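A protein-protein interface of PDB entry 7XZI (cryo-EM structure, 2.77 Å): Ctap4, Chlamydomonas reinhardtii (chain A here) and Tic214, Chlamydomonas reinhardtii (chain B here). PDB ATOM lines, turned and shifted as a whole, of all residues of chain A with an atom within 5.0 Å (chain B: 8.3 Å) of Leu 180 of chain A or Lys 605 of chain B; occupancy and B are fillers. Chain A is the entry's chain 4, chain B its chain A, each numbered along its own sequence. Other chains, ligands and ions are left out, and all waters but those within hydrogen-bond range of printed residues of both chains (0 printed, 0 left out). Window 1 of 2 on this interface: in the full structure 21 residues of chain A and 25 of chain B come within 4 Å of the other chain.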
ATOM      1  N   LYS A 178     -14.759   0.240  -1.174  1.00  0.00           N
ATOM      2  CA  LYS A 178     -13.528  -0.009  -0.440  1.00  0.00           C
ATOM      3  C   LYS A 178     -12.404   0.823  -1.037  1.00  0.00           C
ATOM      4  O   LYS A 178     -12.427   1.166  -2.223  1.00  0.00           O
ATOM      5  CB  LYS A 178     -13.159  -1.498  -0.462  1.00  0.00           C
ATOM      6  CG  LYS A 178     -14.217  -2.414   0.142  1.00  0.00           C
ATOM      7  CD  LYS A 178     -13.962  -3.869  -0.207  1.00  0.00           C
ATOM      8  CE  LYS A 178     -14.047  -4.100  -1.706  1.00  0.00           C
ATOM      9  NZ  LYS A 178     -15.414  -3.828  -2.226  1.00  0.00           N
ATOM     10  N   VAL A 179     -11.420   1.151  -0.197  1.00  0.00           N
ATOM     11  CA  VAL A 179     -10.247   1.884  -0.652  1.00  0.00           C
ATOM     12  C   VAL A 179      -9.383   0.974  -1.514  1.00  0.00           C
ATOM     13  O   VAL A 179      -9.271  -0.231  -1.256  1.00  0.00           O
ATOM     14  CB  VAL A 179      -9.457   2.424   0.553  1.00  0.00           C
ATOM     15  CG1 VAL A 179      -8.385   3.403   0.098  1.00  0.00           C
ATOM     16  CG2 VAL A 179     -10.397   3.075   1.555  1.00  0.00           C
ATOM     17  N   LEU A 180      -8.761   1.545  -2.545  1.00  0.00           N
ATOM     18  CA  LEU A 180      -7.957   0.773  -3.487  1.00  0.00           C
ATOM     19  C   LEU A 180      -6.545   1.337  -3.541  1.00  0.00           C
ATOM     20  O   LEU A 180      -6.355   2.522  -3.824  1.00  0.00           O
ATOM     21  CB  LEU A 180      -8.590   0.780  -4.880  1.00  0.00           C
ATOM     22  CG  LEU A 180      -9.981   0.156  -5.007  1.00  0.00           C
ATOM     23  CD1 LEU A 180     -10.465   0.203  -6.449  1.00  0.00           C
ATOM     24  CD2 LEU A 180      -9.984  -1.272  -4.485  1.00  0.00           C
ATOM     25  N   TYR A 181      -5.556   0.489  -3.273  1.00  0.00           N
ATOM     26  CA  TYR A 181      -4.163   0.894  -3.398  1.00  0.00           C
ATOM     27  C   TYR A 181      -3.726   0.805  -4.855  1.00  0.00           C
ATOM     28  O   TYR A 181      -3.964  -0.209  -5.519  1.00  0.00           O
ATOM     29  CB  TYR A 181      -3.273   0.015  -2.521  1.00  0.00           C
ATOM     30  CG  TYR A 181      -1.796   0.225  -2.752  1.00  0.00           C
ATOM     31  CD1 TYR A 181      -1.138   1.317  -2.206  1.00  0.00           C
ATOM     32  CD2 TYR A 181      -1.058  -0.669  -3.517  1.00  0.00           C
ATOM     33  CE1 TYR A 181       0.210   1.515  -2.415  1.00  0.00           C
ATOM     34  CE2 TYR A 181       0.292  -0.478  -3.731  1.00  0.00           C
ATOM     35  CZ  TYR A 181       0.920   0.614  -3.178  1.00  0.00           C
ATOM     36  OH  TYR A 181       2.265   0.810  -3.387  1.00  0.00           O
ATOM     37  N   ASN A 182      -3.086   1.861  -5.353  1.00  0.00           N
ATOM     38  CA  ASN A 182      -2.556   1.897  -6.708  1.00  0.00           C
ATOM     39  C   ASN A 182      -1.037   1.848  -6.628  1.00  0.00           C
ATOM     40  O   ASN A 182      -0.412   2.743  -6.044  1.00  0.00           O
ATOM     41  CB  ASN A 182      -3.022   3.151  -7.446  1.00  0.00           C
ATOM     42  CG  ASN A 182      -2.619   3.154  -8.907  1.00  0.00           C
ATOM     43  OD1 ASN A 182      -1.563   3.670  -9.271  1.00  0.00           O
ATOM     44  ND2 ASN A 182      -3.461   2.575  -9.753  1.00  0.00           N
ATOM     45  N   LEU A 187      -0.197   5.135  -4.371  1.00  0.00           N
ATOM     46  CA  LEU A 187      -1.069   6.009  -3.596  1.00  0.00           C
ATOM     47  C   LEU A 187      -2.400   5.324  -3.323  1.00  0.00           C
ATOM     48  O   LEU A 187      -2.827   4.434  -4.063  1.00  0.00           O
ATOM     49  CB  LEU A 187      -1.316   7.344  -4.315  1.00  0.00           C
ATOM     50  CG  LEU A 187      -0.146   8.326  -4.397  1.00  0.00           C
ATOM     51  CD1 LEU A 187      -0.541   9.560  -5.192  1.00  0.00           C
ATOM     52  CD2 LEU A 187       0.331   8.711  -3.006  1.00  0.00           C
ATOM     53  N   LEU A 188      -3.054   5.751  -2.248  1.00  0.00           N
ATOM     54  CA  LEU A 188      -4.392   5.267  -1.954  1.00  0.00           C
ATOM     55  C   LEU A 188      -5.423   5.983  -2.820  1.00  0.00           C
ATOM     56  O   LEU A 188      -5.243   7.138  -3.214  1.00  0.00           O
ATOM     57  CB  LEU A 188      -4.723   5.471  -0.475  1.00  0.00           C
ATOM     58  CG  LEU A 188      -3.925   4.640   0.530  1.00  0.00           C
ATOM     59  CD1 LEU A 188      -4.382   4.944   1.945  1.00  0.00           C
ATOM     60  CD2 LEU A 188      -4.070   3.160   0.222  1.00  0.00           C
ATOM     61  N   GLU A 189      -6.514   5.283  -3.113  1.00  0.00           N
ATOM     62  CA  GLU A 189      -7.658   5.839  -3.825  1.00  0.00           C
ATOM     63  C   GLU A 189      -8.887   5.535  -2.979  1.00  0.00           C
ATOM     64  O   GLU A 189      -9.373   4.397  -2.958  1.00  0.00           O
ATOM     65  CB  GLU A 189      -7.783   5.257  -5.230  1.00  0.00           C
ATOM     66  CG  GLU A 189      -6.598   5.536  -6.137  1.00  0.00           C
ATOM     67  CD  GLU A 189      -6.833   5.056  -7.554  1.00  0.00           C
ATOM     68  OE1 GLU A 189      -7.961   4.608  -7.850  1.00  0.00           O
ATOM     69  OE2 GLU A 189      -5.893   5.125  -8.373  1.00  0.00           O
ATOM     70  N   TYR A 236     -19.694 -11.431  -2.028  1.00  0.00           N
ATOM     71  CA  TYR A 236     -18.371 -11.665  -1.453  1.00  0.00           C
ATOM     72  C   TYR A 236     -18.409 -12.682  -0.318  1.00  0.00           C
ATOM     73  O   TYR A 236     -17.471 -13.472  -0.159  1.00  0.00           O
ATOM     74  CB  TYR A 236     -17.767 -10.346  -0.968  1.00  0.00           C
ATOM     75  CG  TYR A 236     -17.126  -9.524  -2.065  1.00  0.00           C
ATOM     76  CD1 TYR A 236     -15.831  -9.789  -2.489  1.00  0.00           C
ATOM     77  CD2 TYR A 236     -17.813  -8.484  -2.673  1.00  0.00           C
ATOM     78  CE1 TYR A 236     -15.240  -9.042  -3.491  1.00  0.00           C
ATOM     79  CE2 TYR A 236     -17.230  -7.732  -3.675  1.00  0.00           C
ATOM     80  CZ  TYR A 236     -15.943  -8.015  -4.079  1.00  0.00           C
ATOM     81  OH  TYR A 236     -15.360  -7.267  -5.076  1.00  0.00           O
ATOM     82  N   ASP A 263     -18.467  -6.930 -10.746  1.00  0.00           N
ATOM     83  CA  ASP A 263     -18.102  -5.562 -10.409  1.00  0.00           C
ATOM     84  C   ASP A 263     -17.199  -4.962 -11.482  1.00  0.00           C
ATOM     85  O   ASP A 263     -16.406  -5.655 -12.122  1.00  0.00           O
ATOM     86  CB  ASP A 263     -17.401  -5.517  -9.051  1.00  0.00           C
ATOM     87  CG  ASP A 263     -18.215  -6.173  -7.955  1.00  0.00           C
ATOM     88  OD1 ASP A 263     -19.259  -6.779  -8.275  1.00  0.00           O
ATOM     89  OD2 ASP A 263     -17.815  -6.081  -6.776  1.00  0.00           O
ATOM     90  N   ASP A 265     -14.505  -1.750 -11.700  1.00  0.00           N
ATOM     91  CA  ASP A 265     -13.733  -0.817 -10.867  1.00  0.00           C
ATOM     92  C   ASP A 265     -14.305  -0.886  -9.451  1.00  0.00           C
ATOM     93  O   ASP A 265     -14.446  -1.991  -8.908  1.00  0.00           O
ATOM     94  CB  ASP A 265     -13.743   0.562 -11.514  1.00  0.00           C
ATOM     95  CG  ASP A 265     -13.290   0.532 -12.962  1.00  0.00           C
ATOM     96  OD1 ASP A 265     -14.007  -0.058 -13.797  1.00  0.00           O
ATOM     97  OD2 ASP A 265     -12.223   1.104 -13.265  1.00  0.00           O
ATOM     98  N   GLU A 266     -14.643   0.241  -8.825  1.00  0.00           N
ATOM     99  CA  GLU A 266     -15.337   0.260  -7.544  1.00  0.00           C
ATOM    100  C   GLU A 266     -16.781   0.728  -7.684  1.00  0.00           C
ATOM    101  O   GLU A 266     -17.468   0.911  -6.675  1.00  0.00           O
ATOM    102  CB  GLU A 266     -14.573   1.149  -6.550  1.00  0.00           C
ATOM    103  CG  GLU A 266     -14.943   0.985  -5.072  1.00  0.00           C
ATOM    104  CD  GLU A 266     -14.810  -0.442  -4.570  1.00  0.00           C
ATOM    105  OE1 GLU A 266     -15.713  -1.263  -4.840  1.00  0.00           O
ATOM    106  OE2 GLU A 266     -13.801  -0.743  -3.900  1.00  0.00           O
ATOM    107  N   PHE B 598      -9.449  -1.460   5.642  1.00  0.00           N
ATOM    108  CA  PHE B 598      -8.950  -2.579   4.856  1.00  0.00           C
ATOM    109  C   PHE B 598      -8.617  -2.084   3.455  1.00  0.00           C
ATOM    110  O   PHE B 598      -9.475  -1.514   2.775  1.00  0.00           O
ATOM    111  CB  PHE B 598      -9.973  -3.712   4.807  1.00  0.00           C
ATOM    112  CG  PHE B 598     -10.060  -4.508   6.077  1.00  0.00           C
ATOM    113  CD1 PHE B 598      -8.915  -4.841   6.782  1.00  0.00           C
ATOM    114  CD2 PHE B 598     -11.287  -4.920   6.571  1.00  0.00           C
ATOM    115  CE1 PHE B 598      -8.993  -5.576   7.951  1.00  0.00           C
ATOM    116  CE2 PHE B 598     -11.371  -5.652   7.740  1.00  0.00           C
ATOM    117  CZ  PHE B 598     -10.222  -5.981   8.431  1.00  0.00           C
ATOM    118  N   ILE B 599      -7.377  -2.304   3.032  1.00  0.00           N
ATOM    119  CA  ILE B 599      -6.889  -1.849   1.736  1.00  0.00           C
ATOM    120  C   ILE B 599      -6.881  -3.030   0.778  1.00  0.00           C
ATOM    121  O   ILE B 599      -6.337  -4.095   1.097  1.00  0.00           O
ATOM    122  CB  ILE B 599      -5.490  -1.223   1.858  1.00  0.00           C
ATOM    123  CG1 ILE B 599      -5.451  -0.229   3.023  1.00  0.00           C
ATOM    124  CG2 ILE B 599      -5.103  -0.533   0.564  1.00  0.00           C
ATOM    125  CD1 ILE B 599      -6.417   0.927   2.878  1.00  0.00           C
ATOM    126  N   TYR B 600      -7.485  -2.847  -0.393  1.00  0.00           N
ATOM    127  CA  TYR B 600      -7.611  -3.895  -1.399  1.00  0.00           C
ATOM    128  C   TYR B 600      -6.887  -3.462  -2.665  1.00  0.00           C
ATOM    129  O   TYR B 600      -7.059  -2.330  -3.126  1.00  0.00           O
ATOM    130  CB  TYR B 600      -9.082  -4.193  -1.701  1.00  0.00           C
ATOM    131  CG  TYR B 600      -9.844  -4.751  -0.521  1.00  0.00           C
ATOM    132  CD1 TYR B 600     -10.341  -3.916   0.469  1.00  0.00           C
ATOM    133  CD2 TYR B 600     -10.067  -6.116  -0.398  1.00  0.00           C
ATOM    134  CE1 TYR B 600     -11.034  -4.423   1.550  1.00  0.00           C
ATOM    135  CE2 TYR B 600     -10.762  -6.631   0.679  1.00  0.00           C
ATOM    136  CZ  TYR B 600     -11.243  -5.781   1.649  1.00  0.00           C
ATOM    137  OH  TYR B 600     -11.936  -6.287   2.724  1.00  0.00           O
ATOM    138  N   SER B 601      -6.077  -4.361  -3.220  1.00  0.00           N
ATOM    139  CA  SER B 601      -5.309  -4.039  -4.415  1.00  0.00           C
ATOM    140  C   SER B 601      -6.233  -3.831  -5.607  1.00  0.00           C
ATOM    141  O   SER B 601      -7.159  -4.616  -5.834  1.00  0.00           O
ATOM    142  CB  SER B 601      -4.303  -5.147  -4.715  1.00  0.00           C
ATOM    143  OG  SER B 601      -3.525  -4.827  -5.855  1.00  0.00           O
ATOM    144  N   LYS B 602      -5.976  -2.769  -6.374  1.00  0.00           N
ATOM    145  CA  LYS B 602      -6.780  -2.493  -7.559  1.00  0.00           C
ATOM    146  C   LYS B 602      -6.556  -3.548  -8.637  1.00  0.00           C
ATOM    147  O   LYS B 602      -7.515  -4.063  -9.226  1.00  0.00           O
ATOM    148  CB  LYS B 602      -6.452  -1.098  -8.095  1.00  0.00           C
ATOM    149  CG  LYS B 602      -7.090  -0.776  -9.434  1.00  0.00           C
ATOM    150  CD  LYS B 602      -6.521   0.508 -10.015  1.00  0.00           C
ATOM    151  CE  LYS B 602      -6.803   1.698  -9.114  1.00  0.00           C
ATOM    152  NZ  LYS B 602      -8.263   1.953  -8.982  1.00  0.00           N
ATOM    153  N   ARG B 603      -5.291  -3.881  -8.907  1.00  0.00           N
ATOM    154  CA  ARG B 603      -4.976  -4.817  -9.982  1.00  0.00           C
ATOM    155  C   ARG B 603      -5.556  -6.196  -9.701  1.00  0.00           C
ATOM    156  O   ARG B 603      -6.195  -6.803 -10.569  1.00  0.00           O
ATOM    157  CB  ARG B 603      -3.461  -4.900 -10.170  1.00  0.00           C
ATOM    158  CG  ARG B 603      -3.024  -5.777 -11.332  1.00  0.00           C
ATOM    159  CD  ARG B 603      -1.556  -6.150 -11.212  1.00  0.00           C
ATOM    160  NE  ARG B 603      -0.727  -4.999 -10.886  1.00  0.00           N
ATOM    161  CZ  ARG B 603      -0.181  -4.188 -11.785  1.00  0.00           C
ATOM    162  NH1 ARG B 603      -0.355  -4.376 -13.083  1.00  0.00           N
ATOM    163  NH2 ARG B 603       0.556  -3.162 -11.370  1.00  0.00           N
ATOM    164  N   TRP B 604      -5.341  -6.709  -8.487  1.00  0.00           N
ATOM    165  CA  TRP B 604      -5.852  -8.030  -8.134  1.00  0.00           C
ATOM    166  C   TRP B 604      -7.374  -8.054  -8.158  1.00  0.00           C
ATOM    167  O   TRP B 604      -7.981  -9.023  -8.633  1.00  0.00           O
ATOM    168  CB  TRP B 604      -5.330  -8.442  -6.757  1.00  0.00           C
ATOM    169  CG  TRP B 604      -3.834  -8.484  -6.669  1.00  0.00           C
ATOM    170  CD1 TRP B 604      -2.951  -8.434  -7.707  1.00  0.00           C
ATOM    171  CD2 TRP B 604      -3.045  -8.579  -5.477  1.00  0.00           C
ATOM    172  NE1 TRP B 604      -1.662  -8.494  -7.237  1.00  0.00           N
ATOM    173  CE2 TRP B 604      -1.693  -8.583  -5.870  1.00  0.00           C
ATOM    174  CE3 TRP B 604      -3.351  -8.661  -4.115  1.00  0.00           C
ATOM    175  CZ2 TRP B 604      -0.648  -8.667  -4.953  1.00  0.00           C
ATOM    176  CZ3 TRP B 604      -2.312  -8.744  -3.206  1.00  0.00           C
ATOM    177  CH2 TRP B 604      -0.977  -8.747  -3.629  1.00  0.00           C
ATOM    178  N   LYS B 605      -8.007  -6.996  -7.649  1.00  0.00           N
ATOM    179  CA  LYS B 605      -9.464  -6.932  -7.651  1.00  0.00           C
ATOM    180  C   LYS B 605     -10.013  -6.936  -9.070  1.00  0.00           C
ATOM    181  O   LYS B 605     -10.968  -7.661  -9.368  1.00  0.00           O
ATOM    182  CB  LYS B 605      -9.939  -5.691  -6.897  1.00  0.00           C
ATOM    183  CG  LYS B 605     -11.448  -5.530  -6.859  1.00  0.00           C
ATOM    184  CD  LYS B 605     -11.849  -4.282  -6.092  1.00  0.00           C
ATOM    185  CE  LYS B 605     -13.360  -4.121  -6.054  1.00  0.00           C
ATOM    186  NZ  LYS B 605     -13.933  -3.927  -7.414  1.00  0.00           N
ATOM    187  N   SER B 606      -9.418  -6.145  -9.963  1.00  0.00           N
ATOM    188  CA  SER B 606      -9.869  -6.128 -11.352  1.00  0.00           C
ATOM    189  C   SER B 606      -9.655  -7.483 -12.016  1.00  0.00           C
ATOM    190  O   SER B 606     -10.521  -7.972 -12.752  1.00  0.00           O
ATOM    191  CB  SER B 606      -9.145  -5.026 -12.126  1.00  0.00           C
ATOM    192  OG  SER B 606      -7.742  -5.223 -12.106  1.00  0.00           O
ATOM    193  N   ILE B 607      -8.502  -8.107 -11.764  1.00  0.00           N
ATOM    194  CA  ILE B 607      -8.194  -9.390 -12.390  1.00  0.00           C
ATOM    195  C   ILE B 607      -9.196 -10.450 -11.954  1.00  0.00           C
ATOM    196  O   ILE B 607      -9.727 -11.206 -12.777  1.00  0.00           O
ATOM    197  CB  ILE B 607      -6.747  -9.809 -12.071  1.00  0.00           C
ATOM    198  CG1 ILE B 607      -5.760  -8.969 -12.883  1.00  0.00           C
ATOM    199  CG2 ILE B 607      -6.541 -11.291 -12.342  1.00  0.00           C
ATOM    200  CD1 ILE B 607      -4.308  -9.327 -12.645  1.00  0.00           C
ATOM    201  N   PHE B 608      -9.485 -10.515 -10.653  1.00  0.00           N
ATOM    202  CA  PHE B 608     -10.431 -11.514 -10.170  1.00  0.00           C
ATOM    203  C   PHE B 608     -11.877 -11.140 -10.463  1.00  0.00           C
ATOM    204  O   PHE B 608     -12.752 -12.010 -10.403  1.00  0.00           O
ATOM    205  CB  PHE B 608     -10.228 -11.754  -8.675  1.00  0.00           C
ATOM    206  CG  PHE B 608      -9.080 -12.667  -8.368  1.00  0.00           C
ATOM    207  CD1 PHE B 608      -9.265 -14.039  -8.318  1.00  0.00           C
ATOM    208  CD2 PHE B 608      -7.811 -12.160  -8.151  1.00  0.00           C
ATOM    209  CE1 PHE B 608      -8.209 -14.886  -8.045  1.00  0.00           C
ATOM    210  CE2 PHE B 608      -6.751 -13.001  -7.878  1.00  0.00           C
ATOM    211  CZ  PHE B 608      -6.949 -14.366  -7.826  1.00  0.00           C
ATOM    212  N   SER B 609     -12.153  -9.872 -10.772  1.00  0.00           N
ATOM    213  CA  SER B 609     -13.489  -9.496 -11.215  1.00  0.00           C
ATOM    214  C   SER B 609     -13.723  -9.887 -12.669  1.00  0.00           C
ATOM    215  O   SER B 609     -14.839 -10.266 -13.041  1.00  0.00           O
ATOM    216  CB  SER B 609     -13.701  -7.995 -11.022  1.00  0.00           C
ATOM    217  OG  SER B 609     -13.573  -7.637  -9.657  1.00  0.00           O
ATOM    218  N   LYS B 610     -12.684  -9.801 -13.504  1.00  0.00           N
ATOM    219  CA  LYS B 610     -12.817 -10.196 -14.902  1.00  0.00           C
ATOM    220  C   LYS B 610     -12.943 -11.702 -15.086  1.00  0.00           C
ATOM    221  O   LYS B 610     -13.281 -12.145 -16.189  1.00  0.00           O
ATOM    222  CB  LYS B 610     -11.627  -9.680 -15.716  1.00  0.00           C
ATOM    223  CG  LYS B 610     -11.630  -8.176 -15.941  1.00  0.00           C
ATOM    224  CD  LYS B 610     -10.595  -7.774 -16.982  1.00  0.00           C
ATOM    225  CE  LYS B 610      -9.186  -8.091 -16.516  1.00  0.00           C
ATOM    226  NZ  LYS B 610      -8.826  -7.321 -15.294  1.00  0.00           N
ATOM    227  N   ILE B 611     -12.683 -12.494 -14.050  1.00  0.00           N
ATOM    228  CA  ILE B 611     -12.782 -13.946 -14.150  1.00  0.00           C
ATOM    229  C   ILE B 611     -14.231 -14.365 -13.942  1.00  0.00           C
ATOM    230  O   ILE B 611     -14.867 -13.980 -12.953  1.00  0.00           O
ATOM    231  CB  ILE B 611     -11.857 -14.628 -13.130  1.00  0.00           C
ATOM    232  CG1 ILE B 611     -10.393 -14.313 -13.444  1.00  0.00           C
ATOM    233  CG2 ILE B 611     -12.093 -16.131 -13.117  1.00  0.00           C
ATOM    234  CD1 ILE B 611      -9.411 -15.029 -12.547  1.00  0.00           C
ATOM    235  N   LYS B 643     -12.756 -15.066  -0.962  1.00  0.00           N
ATOM    236  CA  LYS B 643     -12.725 -14.064  -2.022  1.00  0.00           C
ATOM    237  C   LYS B 643     -12.210 -12.728  -1.503  1.00  0.00           C
ATOM    238  O   LYS B 643     -11.462 -12.029  -2.198  1.00  0.00           O
ATOM    239  CB  LYS B 643     -14.117 -13.909  -2.636  1.00  0.00           C
ATOM    240  CG  LYS B 643     -14.135 -13.107  -3.928  1.00  0.00           C
ATOM    241  CD  LYS B 643     -15.518 -13.107  -4.561  1.00  0.00           C
ATOM    242  CE  LYS B 643     -15.984 -14.519  -4.877  1.00  0.00           C
ATOM    243  NZ  LYS B 643     -17.351 -14.531  -5.467  1.00  0.00           N
ATOM    244  N   THR B 646      -8.500 -12.984  -0.881  1.00  0.00           N
ATOM    245  CA  THR B 646      -7.760 -13.144  -2.128  1.00  0.00           C
ATOM    246  C   THR B 646      -7.318 -11.794  -2.685  1.00  0.00           C
ATOM    247  O   THR B 646      -6.167 -11.631  -3.106  1.00  0.00           O
ATOM    248  CB  THR B 646      -8.613 -13.895  -3.149  1.00  0.00           C
ATOM    249  OG1 THR B 646      -8.963 -15.182  -2.626  1.00  0.00           O
ATOM    250  CG2 THR B 646      -7.849 -14.076  -4.447  1.00  0.00           C
ATOM    251  N   ILE B 647      -8.224 -10.811  -2.692  1.00  0.00           N
ATOM    252  CA  ILE B 647      -7.920  -9.492  -3.239  1.00  0.00           C
ATOM    253  C   ILE B 647      -7.394  -8.526  -2.188  1.00  0.00           C
ATOM    254  O   ILE B 647      -7.053  -7.385  -2.527  1.00  0.00           O
ATOM    255  CB  ILE B 647      -9.161  -8.879  -3.918  1.00  0.00           C
ATOM    256  CG1 ILE B 647     -10.291  -8.712  -2.900  1.00  0.00           C
ATOM    257  CG2 ILE B 647      -9.612  -9.741  -5.088  1.00  0.00           C
ATOM    258  CD1 ILE B 647     -11.538  -8.073  -3.464  1.00  0.00           C
ATOM    259  N   ASN B 648      -7.334  -8.937  -0.923  1.00  0.00           N
ATOM    260  CA  ASN B 648      -6.843  -8.056   0.128  1.00  0.00           C
ATOM    261  C   ASN B 648      -5.359  -7.769  -0.063  1.00  0.00           C
ATOM    262  O   ASN B 648      -4.565  -8.668  -0.352  1.00  0.00           O
ATOM    263  CB  ASN B 648      -7.087  -8.687   1.502  1.00  0.00           C
ATOM    264  CG  ASN B 648      -6.928  -7.696   2.644  1.00  0.00           C
ATOM    265  OD1 ASN B 648      -6.118  -6.773   2.579  1.00  0.00           O
ATOM    266  ND2 ASN B 648      -7.706  -7.890   3.702  1.00  0.00           N
ATOM    267  N   GLN B 649      -4.988  -6.502   0.101  1.00  0.00           N
ATOM    268  CA  GLN B 649      -3.588  -6.085   0.090  1.00  0.00           C
ATOM    269  C   GLN B 649      -3.068  -6.195   1.517  1.00  0.00           C
ATOM    270  O   GLN B 649      -3.369  -5.352   2.365  1.00  0.00           O
ATOM    271  CB  GLN B 649      -3.449  -4.666  -0.452  1.00  0.00           C
ATOM    272  CG  GLN B 649      -2.021  -4.145  -0.482  1.00  0.00           C
ATOM    273  CD  GLN B 649      -1.231  -4.665  -1.666  1.00  0.00           C
ATOM    274  OE1 GLN B 649      -1.753  -4.771  -2.775  1.00  0.00           O
ATOM    275  NE2 GLN B 649       0.036  -4.989  -1.438  1.00  0.00           N
ATOM    276  N   LEU B 659       0.938   5.183   4.348  1.00  0.00           N
ATOM    277  CA  LEU B 659       0.266   5.397   3.069  1.00  0.00           C
ATOM    278  C   LEU B 659      -0.818   6.460   3.188  1.00  0.00           C
ATOM    279  O   LEU B 659      -0.979   7.294   2.290  1.00  0.00           O
ATOM    280  CB  LEU B 659      -0.327   4.084   2.557  1.00  0.00           C
ATOM    281  CG  LEU B 659       0.598   3.169   1.755  1.00  0.00           C
ATOM    282  CD1 LEU B 659      -0.116   1.880   1.387  1.00  0.00           C
ATOM    283  CD2 LEU B 659       1.090   3.883   0.508  1.00  0.00           C
ATOM    284  N   THR B 663      -0.759   9.902   1.057  1.00  0.00           N
ATOM    285  CA  THR B 663      -1.877  10.307   0.211  1.00  0.00           C
ATOM    286  C   THR B 663      -2.426  11.662   0.638  1.00  0.00           C
ATOM    287  O   THR B 663      -2.786  12.487  -0.209  1.00  0.00           O
ATOM    288  CB  THR B 663      -2.976   9.245   0.246  1.00  0.00           C
ATOM    289  OG1 THR B 663      -2.420   7.972  -0.106  1.00  0.00           O
ATOM    290  CG2 THR B 663      -4.083   9.590  -0.736  1.00  0.00           C
ATOM    291  N   LEU B1487       0.186 -13.401 -10.385  1.00  0.00           N
ATOM    292  CA  LEU B1487      -0.749 -12.434 -10.954  1.00  0.00           C
ATOM    293  C   LEU B1487      -0.027 -11.384 -11.792  1.00  0.00           C
ATOM    294  O   LEU B1487      -0.513 -10.990 -12.861  1.00  0.00           O
ATOM    295  CB  LEU B1487      -1.562 -11.772  -9.843  1.00  0.00           C
ATOM    296  CG  LEU B1487      -2.520 -12.676  -9.063  1.00  0.00           C
ATOM    297  CD1 LEU B1487      -3.199 -11.908  -7.942  1.00  0.00           C
ATOM    298  CD2 LEU B1487      -3.553 -13.288  -9.994  1.00  0.00           C
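The side-chain carboxylate (OE1) of Glu 189 of chain A is in salt-bridge range of the side-chain amino group (NZ) of Lys 602 of chain B (2.9 Å).
O of Asp 265 of chain A is in hydrogen-bond range of NZ of Lys 605 of chain B, at 2.5 Å.
The backbone carbonyl oxygen of Tyr 600 of chain B is in hydrogen-bond range of the backbone NH of Tyr 181 of chain A, 3.2 Å away.
The backbone carbonyl oxygen (O) of Tyr 181 of chain A sits at hydrogen-bond distance from the backbone NH (N) of Lys 602 of chain B (3.4 Å).
O of Val 179 of chain A sits at hydrogen-bond distance from N of Tyr 600 of chain B (3.3 Å).
The backbone NH (N) of Leu 188 of chain A is in hydrogen-bond range of the side-chain hydroxyl (OG1) of Thr 663 of chain B, at 3.2 Å.
The backbone carbonyl oxygen (O) of Lys 602 of chain B lies within hydrogen-bond range of the side-chain hydroxyl (OG) of Ser 606 of chain B.
The backbone carbonyl oxygen of Leu 187 of chain A sits at hydrogen-bond distance from the backbone NH of Asn 182 of chain A, 2.9 Å away.
The backbone NH of Ser 601 of chain B is in hydrogen-bond range of the backbone carbonyl oxygen of Ile 647 of chain B, at 3.3 Å.
The backbone carbonyl oxygen of Ile 599 of chain B lies within hydrogen-bond range of the backbone NH of Gln 649 of chain B, 2.9 Å away.
The backbone carbonyl oxygen (O) of Ile 599 of chain B sits close to the side-chain amide oxygen (OD1) of Asn 648 of chain B.
N of Glu 189 of chain A lies within hydrogen-bond range of O of Leu 180 of chain A, 2.9 Å away.
Printed residues of chain A that touch a printed residue of chain B: Lys 178, Val 179, Leu 180, Tyr 181, Asn 182, Leu 188, Glu 189, Tyr 236, Asp 263, Asp 265 and Glu 266.
Hydrophobic or aromatic side chains of chain A that line the printed part of chain B: Leu 180, Tyr 181, Leu 188 and Tyr 236.
Of the 22 printed residues of chain B, 9 touch a printed residue of chain A.
Hydrophobic or aromatic side chains of chain B that line the printed part of chain A: Ile 599, Tyr 600, Ile 647 and Leu 659.
Among the printed residues, Asp or Glu carboxylates within 4 Å of a Lys or Arg side-chain nitrogen of the other chain: Glu 189 of chain A with Lys 602 of chain B (2.9 Å).
Lys 178 of chain A touches Tyr 600 of chain B.
Tyr 600 of chain B touches Leu 180 of chain A.
Leu 180 of chain A touches Lys 602 of chain B.
Lys 605 of chain B touches Leu 180 of chain A (CD to CD2, 3.9 Å).
Tyr 181 of chain A touches Ile 599 of chain B.
Tyr 181 of chain A touches Leu 659 of chain B.
CD2 of Leu 188 of chain A touches CG2 of Ile 599 of chain B, at 3.8 Å.
Tyr 236 of chain A touches Lys 605 of chain B (OH to CE, 3.9 Å).
CE1 of Tyr 236 of chain A touches CD1 of Ile 647 of chain B, at 3.8 Å.
OE1 of Glu 266 of chain A touches CE of Lys 605 of chain B, 3.9 Å away.
Leu 180 of chain A touches just these residues of chain B: Tyr 600 (3.3 Å), Lys 602 (3.8 Å) and Lys 605 (3.9 Å).
Lys 605 of chain B touches four residues of chain A.
Printed residues of chain A within 4 Å of Ile 599 of chain B: Tyr 181 (3.6 Å) and Leu 188 (3.8 Å).
Of the printed residues of chain B, Tyr 181 of chain A touches Ile 599, Tyr 600, Lys 602 and Leu 659.
Printed residues of chain B within 4 Å of Leu 188 of chain A: Ile 599 and Thr 663.
Of the printed residues of chain B, Lys 178 of chain A touches Tyr 600 (3.5 Å).
Of the printed residues of chain A, Ser 609 of chain B touches Asp 263.
Leu 1487 of chain B touches none of the printed residues of chain A.
Gln 649 of chain B touches none of the printed residues of chain A.
The nearest residue of chain B that does not touch Leu 180 of chain A is Ser 601 of chain B (4.6 Å).
The nearest printed residue of chain A that does not touch Thr 663 of chain B is Leu 187 of chain A (4.1 Å).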
